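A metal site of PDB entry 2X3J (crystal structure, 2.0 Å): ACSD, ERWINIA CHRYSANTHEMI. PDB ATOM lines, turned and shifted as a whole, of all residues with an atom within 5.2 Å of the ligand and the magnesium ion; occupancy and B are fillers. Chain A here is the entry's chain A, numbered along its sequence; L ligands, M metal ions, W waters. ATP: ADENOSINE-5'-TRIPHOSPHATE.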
ATOM      1  N   LEU A 166     -14.038   3.086  28.577  1.00  0.00           N
ATOM      2  CA  LEU A 166     -13.679   3.403  27.200  1.00  0.00           C
ATOM      3  C   LEU A 166     -14.694   2.713  26.286  1.00  0.00           C
ATOM      4  O   LEU A 166     -14.356   1.756  25.550  1.00  0.00           O
ATOM      5  CB  LEU A 166     -12.246   2.996  26.852  1.00  0.00           C
ATOM      6  CG  LEU A 166     -11.548   3.565  25.598  1.00  0.00           C
ATOM      7  CD1 LEU A 166     -11.243   5.055  25.695  1.00  0.00           C
ATOM      8  CD2 LEU A 166     -10.259   2.809  25.332  1.00  0.00           C
ATOM      9  N   GLY A 169     -13.748   2.646  22.496  1.00  0.00           N
ATOM     10  CA  GLY A 169     -12.407   2.182  22.188  1.00  0.00           C
ATOM     11  C   GLY A 169     -11.607   3.178  21.379  1.00  0.00           C
ATOM     12  O   GLY A 169     -11.958   4.347  21.280  1.00  0.00           O
ATOM     13  N   HIS A 170     -10.520   2.685  20.794  1.00  0.00           N
ATOM     14  CA  HIS A 170      -9.717   3.458  19.847  1.00  0.00           C
ATOM     15  C   HIS A 170     -10.596   4.272  18.887  1.00  0.00           C
ATOM     16  O   HIS A 170     -11.413   3.721  18.140  1.00  0.00           O
ATOM     17  CB  HIS A 170      -8.802   2.500  19.075  1.00  0.00           C
ATOM     18  CG  HIS A 170      -7.610   3.158  18.455  1.00  0.00           C
ATOM     19  ND1 HIS A 170      -7.684   4.326  17.722  1.00  0.00           N
ATOM     20  CD2 HIS A 170      -6.312   2.765  18.419  1.00  0.00           C
ATOM     21  CE1 HIS A 170      -6.482   4.638  17.263  1.00  0.00           C
ATOM     22  NE2 HIS A 170      -5.631   3.701  17.659  1.00  0.00           N
ATOM     23  N   PRO A 171     -10.432   5.607  18.909  1.00  0.00           N
ATOM     24  CA  PRO A 171     -11.368   6.437  18.164  1.00  0.00           C
ATOM     25  C   PRO A 171     -11.119   6.486  16.657  1.00  0.00           C
ATOM     26  O   PRO A 171     -11.937   7.045  15.919  1.00  0.00           O
ATOM     27  CB  PRO A 171     -11.197   7.833  18.790  1.00  0.00           C
ATOM     28  CG  PRO A 171      -9.814   7.825  19.392  1.00  0.00           C
ATOM     29  CD  PRO A 171      -9.398   6.395  19.616  1.00  0.00           C
ATOM     30  N   PRO A 176     -12.773  -1.240  16.915  1.00  0.00           N
ATOM     31  CA  PRO A 176     -12.035  -1.136  18.185  1.00  0.00           C
ATOM     32  C   PRO A 176     -12.394  -2.176  19.252  1.00  0.00           C
ATOM     33  O   PRO A 176     -11.639  -2.360  20.210  1.00  0.00           O
ATOM     34  CB  PRO A 176     -12.394   0.269  18.682  1.00  0.00           C
ATOM     35  CG  PRO A 176     -13.726   0.576  18.026  1.00  0.00           C
ATOM     36  CD  PRO A 176     -13.583  -0.038  16.662  1.00  0.00           C
ATOM     37  N   THR A 277      -8.403  -4.454  32.580  1.00  0.00           N
ATOM     38  CA  THR A 277      -8.310  -3.056  32.181  1.00  0.00           C
ATOM     39  C   THR A 277      -8.630  -2.971  30.690  1.00  0.00           C
ATOM     40  O   THR A 277      -8.984  -3.971  30.074  1.00  0.00           O
ATOM     41  CB  THR A 277      -6.902  -2.494  32.490  1.00  0.00           C
ATOM     42  OG1 THR A 277      -5.925  -3.254  31.775  1.00  0.00           O
ATOM     43  CG2 THR A 277      -6.593  -2.620  33.990  1.00  0.00           C
ATOM     44  N   ALA A 278      -8.496  -1.773  30.115  1.00  0.00           N
ATOM     45  CA  ALA A 278      -8.803  -1.532  28.717  1.00  0.00           C
ATOM     46  C   ALA A 278      -7.968  -2.362  27.757  1.00  0.00           C
ATOM     47  O   ALA A 278      -8.406  -2.667  26.669  1.00  0.00           O
ATOM     48  CB  ALA A 278      -8.677  -0.062  28.394  1.00  0.00           C
ATOM     49  N   SER A 279      -6.757  -2.742  28.154  1.00  0.00           N
ATOM     50  CA  SER A 279      -5.951  -3.604  27.293  1.00  0.00           C
ATOM     51  C   SER A 279      -6.335  -5.103  27.348  1.00  0.00           C
ATOM     52  O   SER A 279      -5.704  -5.929  26.691  1.00  0.00           O
ATOM     53  CB  SER A 279      -4.470  -3.411  27.584  1.00  0.00           C
ATOM     54  OG  SER A 279      -4.135  -3.943  28.850  1.00  0.00           O
ATOM     55  N   ARG A 281      -5.893  -7.952  28.553  1.00  0.00           N
ATOM     56  CA  ARG A 281      -5.022  -8.957  29.172  1.00  0.00           C
ATOM     57  C   ARG A 281      -4.188  -8.460  30.358  1.00  0.00           C
ATOM     58  O   ARG A 281      -3.360  -9.207  30.906  1.00  0.00           O
ATOM     59  CB  ARG A 281      -4.143  -9.666  28.124  1.00  0.00           C
ATOM     60  CG  ARG A 281      -3.492  -8.781  27.068  1.00  0.00           C
ATOM     61  CD  ARG A 281      -2.433  -7.825  27.609  1.00  0.00           C
ATOM     62  NE  ARG A 281      -1.491  -7.368  26.571  1.00  0.00           N
ATOM     63  CZ  ARG A 281      -0.389  -8.021  26.202  1.00  0.00           C
ATOM     64  NH1 ARG A 281      -0.058  -9.181  26.775  1.00  0.00           N
ATOM     65  NH2 ARG A 281       0.388  -7.523  25.264  1.00  0.00           N
ATOM     66  N   THR A 282      -4.373  -7.198  30.734  1.00  0.00           N
ATOM     67  CA  THR A 282      -3.801  -6.651  31.975  1.00  0.00           C
ATOM     68  C   THR A 282      -4.919  -6.419  32.994  1.00  0.00           C
ATOM     69  O   THR A 282      -5.935  -5.756  32.686  1.00  0.00           O
ATOM     70  CB  THR A 282      -3.010  -5.347  31.722  1.00  0.00           C
ATOM     71  OG1 THR A 282      -1.978  -5.608  30.743  1.00  0.00           O
ATOM     72  CG2 THR A 282      -2.314  -4.827  33.010  1.00  0.00           C
ATOM     73  N   LYS A 293      -0.164  -8.567  34.037  1.00  0.00           N
ATOM     74  CA  LYS A 293      -0.255  -8.591  32.591  1.00  0.00           C
ATOM     75  C   LYS A 293       0.135  -9.987  32.097  1.00  0.00           C
ATOM     76  O   LYS A 293       1.211 -10.473  32.408  1.00  0.00           O
ATOM     77  CB  LYS A 293       0.639  -7.511  31.982  1.00  0.00           C
ATOM     78  CG  LYS A 293       0.867  -7.624  30.477  1.00  0.00           C
ATOM     79  CD  LYS A 293       1.634  -6.416  29.967  1.00  0.00           C
ATOM     80  CE  LYS A 293       1.710  -6.460  28.444  1.00  0.00           C
ATOM     81  NZ  LYS A 293       2.367  -5.226  27.926  1.00  0.00           N
ATOM     82  N   ILE A 300      -6.540  -8.343  19.100  1.00  0.00           N
ATOM     83  CA  ILE A 300      -7.304  -7.215  19.588  1.00  0.00           C
ATOM     84  C   ILE A 300      -6.710  -5.986  18.932  1.00  0.00           C
ATOM     85  O   ILE A 300      -5.495  -5.727  19.022  1.00  0.00           O
ATOM     86  CB  ILE A 300      -7.215  -7.069  21.134  1.00  0.00           C
ATOM     87  CG1 ILE A 300      -7.732  -8.348  21.828  1.00  0.00           C
ATOM     88  CG2 ILE A 300      -7.991  -5.810  21.596  1.00  0.00           C
ATOM     89  CD1 ILE A 300      -7.200  -8.554  23.226  1.00  0.00           C
ATOM     90  N   THR A 301      -7.588  -5.208  18.283  1.00  0.00           N
ATOM     91  CA  THR A 301      -7.181  -4.184  17.327  1.00  0.00           C
ATOM     92  C   THR A 301      -6.065  -4.731  16.440  1.00  0.00           C
ATOM     93  O   THR A 301      -6.239  -5.818  15.879  1.00  0.00           O
ATOM     94  CB  THR A 301      -6.921  -2.773  17.970  1.00  0.00           C
ATOM     95  OG1 THR A 301      -5.927  -2.854  18.995  1.00  0.00           O
ATOM     96  CG2 THR A 301      -8.222  -2.188  18.539  1.00  0.00           C
ATOM     97  N   ARG A 305      -2.094 -10.407  21.131  1.00  0.00           N
ATOM     98  CA  ARG A 305      -1.686  -9.825  22.416  1.00  0.00           C
ATOM     99  C   ARG A 305      -0.898 -10.811  23.304  1.00  0.00           C
ATOM    100  O   ARG A 305      -1.133 -10.926  24.503  1.00  0.00           O
ATOM    101  CB  ARG A 305      -2.911  -9.217  23.118  1.00  0.00           C
ATOM    102  CG  ARG A 305      -3.641  -8.134  22.326  1.00  0.00           C
ATOM    103  CD  ARG A 305      -2.708  -6.954  21.992  1.00  0.00           C
ATOM    104  NE  ARG A 305      -3.318  -5.984  21.087  1.00  0.00           N
ATOM    105  CZ  ARG A 305      -2.783  -4.810  20.761  1.00  0.00           C
ATOM    106  NH1 ARG A 305      -1.600  -4.455  21.279  1.00  0.00           N
ATOM    107  NH2 ARG A 305      -3.414  -3.987  19.934  1.00  0.00           N
ATOM    108  N   ARG A 369       3.281  -5.136  36.729  1.00  0.00           N
ATOM    109  CA  ARG A 369       3.459  -3.703  36.586  1.00  0.00           C
ATOM    110  C   ARG A 369       3.074  -3.070  37.917  1.00  0.00           C
ATOM    111  O   ARG A 369       2.061  -3.428  38.498  1.00  0.00           O
ATOM    112  CB  ARG A 369       2.595  -3.142  35.453  1.00  0.00           C
ATOM    113  CG  ARG A 369       2.610  -1.625  35.318  1.00  0.00           C
ATOM    114  CD  ARG A 369       1.757  -1.123  34.140  1.00  0.00           C
ATOM    115  NE  ARG A 369       2.319  -1.592  32.877  1.00  0.00           N
ATOM    116  CZ  ARG A 369       1.640  -2.187  31.899  1.00  0.00           C
ATOM    117  NH1 ARG A 369       0.317  -2.327  31.983  1.00  0.00           N
ATOM    118  NH2 ARG A 369       2.290  -2.620  30.816  1.00  0.00           N
ATOM    119  N   GLU A 442       6.109   4.567  23.537  1.00  0.00           N
ATOM    120  CA  GLU A 442       4.918   4.508  22.685  1.00  0.00           C
ATOM    121  C   GLU A 442       3.784   5.273  23.384  1.00  0.00           C
ATOM    122  O   GLU A 442       2.872   4.670  23.928  1.00  0.00           O
ATOM    123  CB  GLU A 442       4.543   3.058  22.379  1.00  0.00           C
ATOM    124  CG  GLU A 442       3.661   2.928  21.122  1.00  0.00           C
ATOM    125  CD  GLU A 442       3.112   1.528  20.853  1.00  0.00           C
ATOM    126  OE1 GLU A 442       3.447   0.568  21.590  1.00  0.00           O
ATOM    127  OE2 GLU A 442       2.327   1.402  19.882  1.00  0.00           O
ATOM    128  N   HIS A 444       0.912   6.571  23.195  1.00  0.00           N
ATOM    129  CA  HIS A 444      -0.469   6.699  22.750  1.00  0.00           C
ATOM    130  C   HIS A 444      -1.400   6.843  23.947  1.00  0.00           C
ATOM    131  O   HIS A 444      -0.957   6.795  25.117  1.00  0.00           O
ATOM    132  CB  HIS A 444      -0.888   5.567  21.785  1.00  0.00           C
ATOM    133  CG  HIS A 444      -0.742   4.180  22.335  1.00  0.00           C
ATOM    134  ND1 HIS A 444      -1.311   3.783  23.524  1.00  0.00           N
ATOM    135  CD2 HIS A 444      -0.112   3.096  21.828  1.00  0.00           C
ATOM    136  CE1 HIS A 444      -1.042   2.499  23.726  1.00  0.00           C
ATOM    137  NE2 HIS A 444      -0.321   2.060  22.709  1.00  0.00           N
ATOM    138  N   LEU A 445      -2.684   7.033  23.673  1.00  0.00           N
ATOM    139  CA  LEU A 445      -3.645   7.389  24.721  1.00  0.00           C
ATOM    140  C   LEU A 445      -3.788   6.342  25.830  1.00  0.00           C
ATOM    141  O   LEU A 445      -3.978   6.700  27.016  1.00  0.00           O
ATOM    142  CB  LEU A 445      -5.008   7.716  24.105  1.00  0.00           C
ATOM    143  CG  LEU A 445      -5.168   9.113  23.504  1.00  0.00           C
ATOM    144  CD1 LEU A 445      -6.470   9.150  22.706  1.00  0.00           C
ATOM    145  CD2 LEU A 445      -5.161  10.198  24.595  1.00  0.00           C
ATOM    146  N   GLN A 446      -3.665   5.076  25.449  1.00  0.00           N
ATOM    147  CA  GLN A 446      -3.790   3.969  26.395  1.00  0.00           C
ATOM    148  C   GLN A 446      -2.534   3.695  27.211  1.00  0.00           C
ATOM    149  O   GLN A 446      -2.605   3.030  28.249  1.00  0.00           O
ATOM    150  CB  GLN A 446      -4.287   2.698  25.701  1.00  0.00           C
ATOM    151  CG  GLN A 446      -4.591   1.513  26.649  1.00  0.00           C
ATOM    152  CD  GLN A 446      -3.346   0.676  26.962  1.00  0.00           C
ATOM    153  OE1 GLN A 446      -2.318   0.788  26.296  1.00  0.00           O
ATOM    154  NE2 GLN A 446      -3.418  -0.131  28.021  1.00  0.00           N
ATOM    155  N   ASN A 447      -1.388   4.181  26.748  1.00  0.00           N
ATOM    156  CA  ASN A 447      -0.150   4.061  27.501  1.00  0.00           C
ATOM    157  C   ASN A 447       0.107   5.263  28.399  1.00  0.00           C
ATOM    158  O   ASN A 447       1.205   5.418  28.927  1.00  0.00           O
ATOM    159  CB  ASN A 447       1.019   3.857  26.537  1.00  0.00           C
ATOM    160  CG  ASN A 447       1.125   2.429  26.049  1.00  0.00           C
ATOM    161  OD1 ASN A 447       0.527   1.508  26.637  1.00  0.00           O
ATOM    162  ND2 ASN A 447       1.886   2.221  24.978  1.00  0.00           N
ATOM    163  N   ARG A 463       3.455   4.247  30.575  1.00  0.00           N
ATOM    164  CA  ARG A 463       3.540   2.828  30.868  1.00  0.00           C
ATOM    165  C   ARG A 463       3.756   1.979  29.620  1.00  0.00           C
ATOM    166  O   ARG A 463       3.648   2.494  28.490  1.00  0.00           O
ATOM    167  CB  ARG A 463       2.289   2.351  31.614  1.00  0.00           C
ATOM    168  CG  ARG A 463       1.002   2.458  30.806  1.00  0.00           C
ATOM    169  CD  ARG A 463      -0.121   1.617  31.382  1.00  0.00           C
ATOM    170  NE  ARG A 463      -1.403   2.023  30.808  1.00  0.00           N
ATOM    171  CZ  ARG A 463      -2.545   2.059  31.467  1.00  0.00           C
ATOM    172  NH1 ARG A 463      -2.587   1.732  32.769  1.00  0.00           N
ATOM    173  NH2 ARG A 463      -3.646   2.457  30.855  1.00  0.00           N
ATOM    174  N   ASP A 464       4.044   0.705  29.852  1.00  0.00           N
ATOM    175  CA  ASP A 464       4.158  -0.350  28.835  1.00  0.00           C
ATOM    176  C   ASP A 464       5.562  -0.429  28.242  1.00  0.00           C
ATOM    177  O   ASP A 464       5.885   0.230  27.252  1.00  0.00           O
ATOM    178  CB  ASP A 464       3.042  -0.221  27.784  1.00  0.00           C
ATOM    179  CG  ASP A 464       2.894  -1.462  26.927  1.00  0.00           C
ATOM    180  OD1 ASP A 464       1.926  -1.494  26.130  1.00  0.00           O
ATOM    181  OD2 ASP A 464       3.721  -2.394  27.037  1.00  0.00           O
ATOM    182  N   GLU A 466       6.989  -3.026  26.983  1.00  0.00           N
ATOM    183  CA  GLU A 466       7.125  -4.092  25.999  1.00  0.00           C
ATOM    184  C   GLU A 466       7.114  -3.491  24.621  1.00  0.00           C
ATOM    185  O   GLU A 466       7.549  -4.134  23.654  1.00  0.00           O
ATOM    186  CB  GLU A 466       5.999  -5.104  26.180  1.00  0.00           C
ATOM    187  CG  GLU A 466       6.008  -5.775  27.573  1.00  0.00           C
ATOM    188  CD  GLU A 466       5.436  -4.867  28.657  1.00  0.00           C
ATOM    189  OE1 GLU A 466       6.009  -3.808  28.906  1.00  0.00           O
ATOM    190  OE2 GLU A 466       4.418  -5.181  29.265  1.00  0.00           O
ATOM    191  N   ASN A 509      -2.296  10.498  17.401  1.00  0.00           N
ATOM    192  CA  ASN A 509      -3.029   9.634  18.319  1.00  0.00           C
ATOM    193  C   ASN A 509      -3.489  10.366  19.576  1.00  0.00           C
ATOM    194  O   ASN A 509      -4.644  10.226  20.012  1.00  0.00           O
ATOM    195  CB  ASN A 509      -2.161   8.408  18.677  1.00  0.00           C
ATOM    196  CG  ASN A 509      -2.830   7.427  19.633  1.00  0.00           C
ATOM    197  OD1 ASN A 509      -2.990   7.715  20.816  1.00  0.00           O
ATOM    198  ND2 ASN A 509      -3.202   6.257  19.132  1.00  0.00           N
HETATM  199  PG  ATP L   1      -0.649  -2.711  28.706  1.00  0.00           P
HETATM  200  O1G ATP L   1      -0.811  -1.257  28.265  1.00  0.00           O
HETATM  201  O2G ATP L   1      -1.525  -3.093  29.900  1.00  0.00           O
HETATM  202  O3G ATP L   1       0.760  -3.251  28.753  1.00  0.00           O
HETATM  203  PB  ATP L   1      -0.783  -3.785  25.986  1.00  0.00           P
HETATM  204  O1B ATP L   1       0.716  -3.982  25.895  1.00  0.00           O
HETATM  205  O2B ATP L   1      -1.678  -4.811  25.304  1.00  0.00           O
HETATM  206  O3B ATP L   1      -1.283  -3.635  27.530  1.00  0.00           O
HETATM  207  PA  ATP L   1      -0.646  -1.788  23.937  1.00  0.00           P
HETATM  208  O1A ATP L   1      -0.128  -0.376  24.157  1.00  0.00           O
HETATM  209  O2A ATP L   1       0.248  -2.830  23.282  1.00  0.00           O
HETATM  210  O3A ATP L   1      -1.211  -2.351  25.349  1.00  0.00           O
HETATM  211  O5' ATP L   1      -1.990  -1.693  23.027  1.00  0.00           O
HETATM  212  C5' ATP L   1      -3.002  -0.754  23.406  1.00  0.00           C
HETATM  213  C4' ATP L   1      -4.325  -1.440  23.771  1.00  0.00           C
HETATM  214  O4' ATP L   1      -5.234  -0.402  24.166  1.00  0.00           O
HETATM  215  C3' ATP L   1      -4.996  -2.107  22.582  1.00  0.00           C
HETATM  216  O3' ATP L   1      -5.783  -3.204  23.053  1.00  0.00           O
HETATM  217  C2' ATP L   1      -5.897  -1.025  21.988  1.00  0.00           C
HETATM  218  O2' ATP L   1      -7.076  -1.546  21.351  1.00  0.00           O
HETATM  219  C1' ATP L   1      -6.299  -0.210  23.200  1.00  0.00           C
HETATM  220  N9  ATP L   1      -6.535   1.227  22.881  1.00  0.00           N
HETATM  221  C8  ATP L   1      -7.642   1.918  23.223  1.00  0.00           C
HETATM  222  N7  ATP L   1      -7.562   3.196  22.793  1.00  0.00           N
HETATM  223  C5  ATP L   1      -6.383   3.347  22.171  1.00  0.00           C
HETATM  224  C6  ATP L   1      -5.683   4.459  21.483  1.00  0.00           C
HETATM  225  N6  ATP L   1      -6.249   5.692  21.360  1.00  0.00           N
HETATM  226  N1  ATP L   1      -4.468   4.188  20.973  1.00  0.00           N
HETATM  227  C2  ATP L   1      -3.901   2.977  21.052  1.00  0.00           C
HETATM  228  N3  ATP L   1      -4.482   1.924  21.657  1.00  0.00           N
HETATM  229  C4  ATP L   1      -5.708   2.060  22.226  1.00  0.00           C
HETATM  230 MG    MG M   1      -0.262  -0.382  26.405  1.00  0.00          MG
HETATM  231  O   HOH W   1      -3.277  -1.612  31.510  1.00  0.00           O
HETATM  232  O   HOH W   2      -9.947  -0.263  21.120  1.00  0.00           O
HETATM  233  O   HOH W   3      -8.392   5.961  23.145  1.00  0.00           O
HETATM  234  O   HOH W   4       2.985  -5.729  25.064  1.00  0.00           O
HETATM  235  O   HOH W   5      -4.232  -5.175  24.190  1.00  0.00           O
HETATM  236  O   HOH W   6      -8.648  -2.813  23.921  1.00  0.00           O
HETATM  237  O   HOH W   7      -6.173   8.130  19.022  1.00  0.00           O
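Three residues have an atom within 4 Å of the magnesium ion: Gln 446, Asn 447 and Asp 464. The nearest printed residue that does not touch the magnesium ion is His 444 (4.01 Å).
The magnesium ion is bound by OD1 of Asn 447 (2.1 Å), O1G of the ligand (2.1 Å), O1A of the ligand (2.3 Å), OE1 of Gln 446 (2.4 Å), O3A of the ligand (2.4 Å) and OD1 of Asp 464 (2.5 Å). The magnesium ion has six donor atoms within binding distance.
Residues that only touch the ligand: His 170 (3.5 Å), Leu 166 (3.5 Å), Leu 445 (3.6 Å), Pro 171 (3.7 Å) and Ile 300 (3.7 Å). Hydrophobic or aromatic side chains that line the ligand: Leu 166, His 170, Pro 171, Ile 300, His 444 and Leu 445. Within 4 Å of the ligand: Leu 166, His 170, Pro 171, Ser 279, Arg 281, Thr 282, Lys 293, Ile 300, Thr 301, Arg 305, Arg 369, His 444, Leu 445, Gln 446, Asn 447, Asp 464 and Asn 509.
ND2 of Asn 447 sits at hydrogen-bond distance from NE2 of His 444 (3.2 Å). A ring nitrogen (ND1) of His 444 lies close to the backbone NH (N) of Gln 446 (3.3 Å). NH2 of Arg 463 sits at hydrogen-bond distance from O of Gln 446. OD2 of Asp 464 is in salt-bridge range of NZ of Lys 293. OD2 of Asp 464 sits close to N of Glu 466 (3.3 Å). NH2 of Arg 369 lies within salt-bridge range of OE2 of Glu 466. NH1 of Arg 281 is in hydrogen-bond range of O of Arg 305 (3.1 Å). The side-chain hydroxyl of Ser 279 lies within hydrogen-bond range of the side-chain hydroxyl of Thr 277 (3.5 Å).
The guanidinium group (NH2) of Arg 369 is in salt-bridge range of an oxygen (O3G) of the ligand (2.6 Å). An oxygen (O3G) of the ligand is in salt-bridge range of the side-chain amino group of Lys 293 (2.7 Å). An oxygen (O2G) of the ligand is in hydrogen-bond range of the side-chain hydroxyl (OG1) of Thr 282 (2.7 Å). An oxygen (O1A) of the ligand lies close to a ring nitrogen (NE2) of His 444, 2.8 Å away. An oxygen (O2B) of the ligand lies within salt-bridge range of the guanidinium group (NE) of Arg 281, 2.9 Å away. O2' of the ligand is in hydrogen-bond range of OG1 of Thr 301 (2.9 Å). The side-chain hydroxyl (OG) of Ser 279 is in hydrogen-bond range of an oxygen (O2G) of the ligand, 2.9 Å away. A nitrogen (N1) of the ligand sits at hydrogen-bond distance from the side-chain amide nitrogen (ND2) of Asn 509 (3.0 Å). An oxygen (O2A) of the ligand lies within salt-bridge range of the guanidinium group (NH1) of Arg 305.
Water W5 lies within hydrogen-bond range of an oxygen (O3') of the ligand (2.8 Å), the backbone carbonyl oxygen of Ser 279 (3.0 Å) and the guanidinium group of Arg 305 (3.3 Å). Water W1 lies within hydrogen-bond range of O2G of the ligand and OG1 of Thr 277. Water W4 lies within hydrogen-bond range of the side-chain amino group of Lys 293, an oxygen (O1B) of the ligand and the guanidinium group of Arg 281. Water W6 bridges O of Ala 278 and O3' of the ligand. Water W2 lies within hydrogen-bond range of O of Pro 176 (2.8 Å), N of His 170 (3.0 Å) and O2' of the ligand (3.2 Å). Water W7 bridges the backbone carbonyl oxygen (O) of Asn 509 (2.8 Å) and a nitrogen (N6) of the ligand (3.4 Å).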
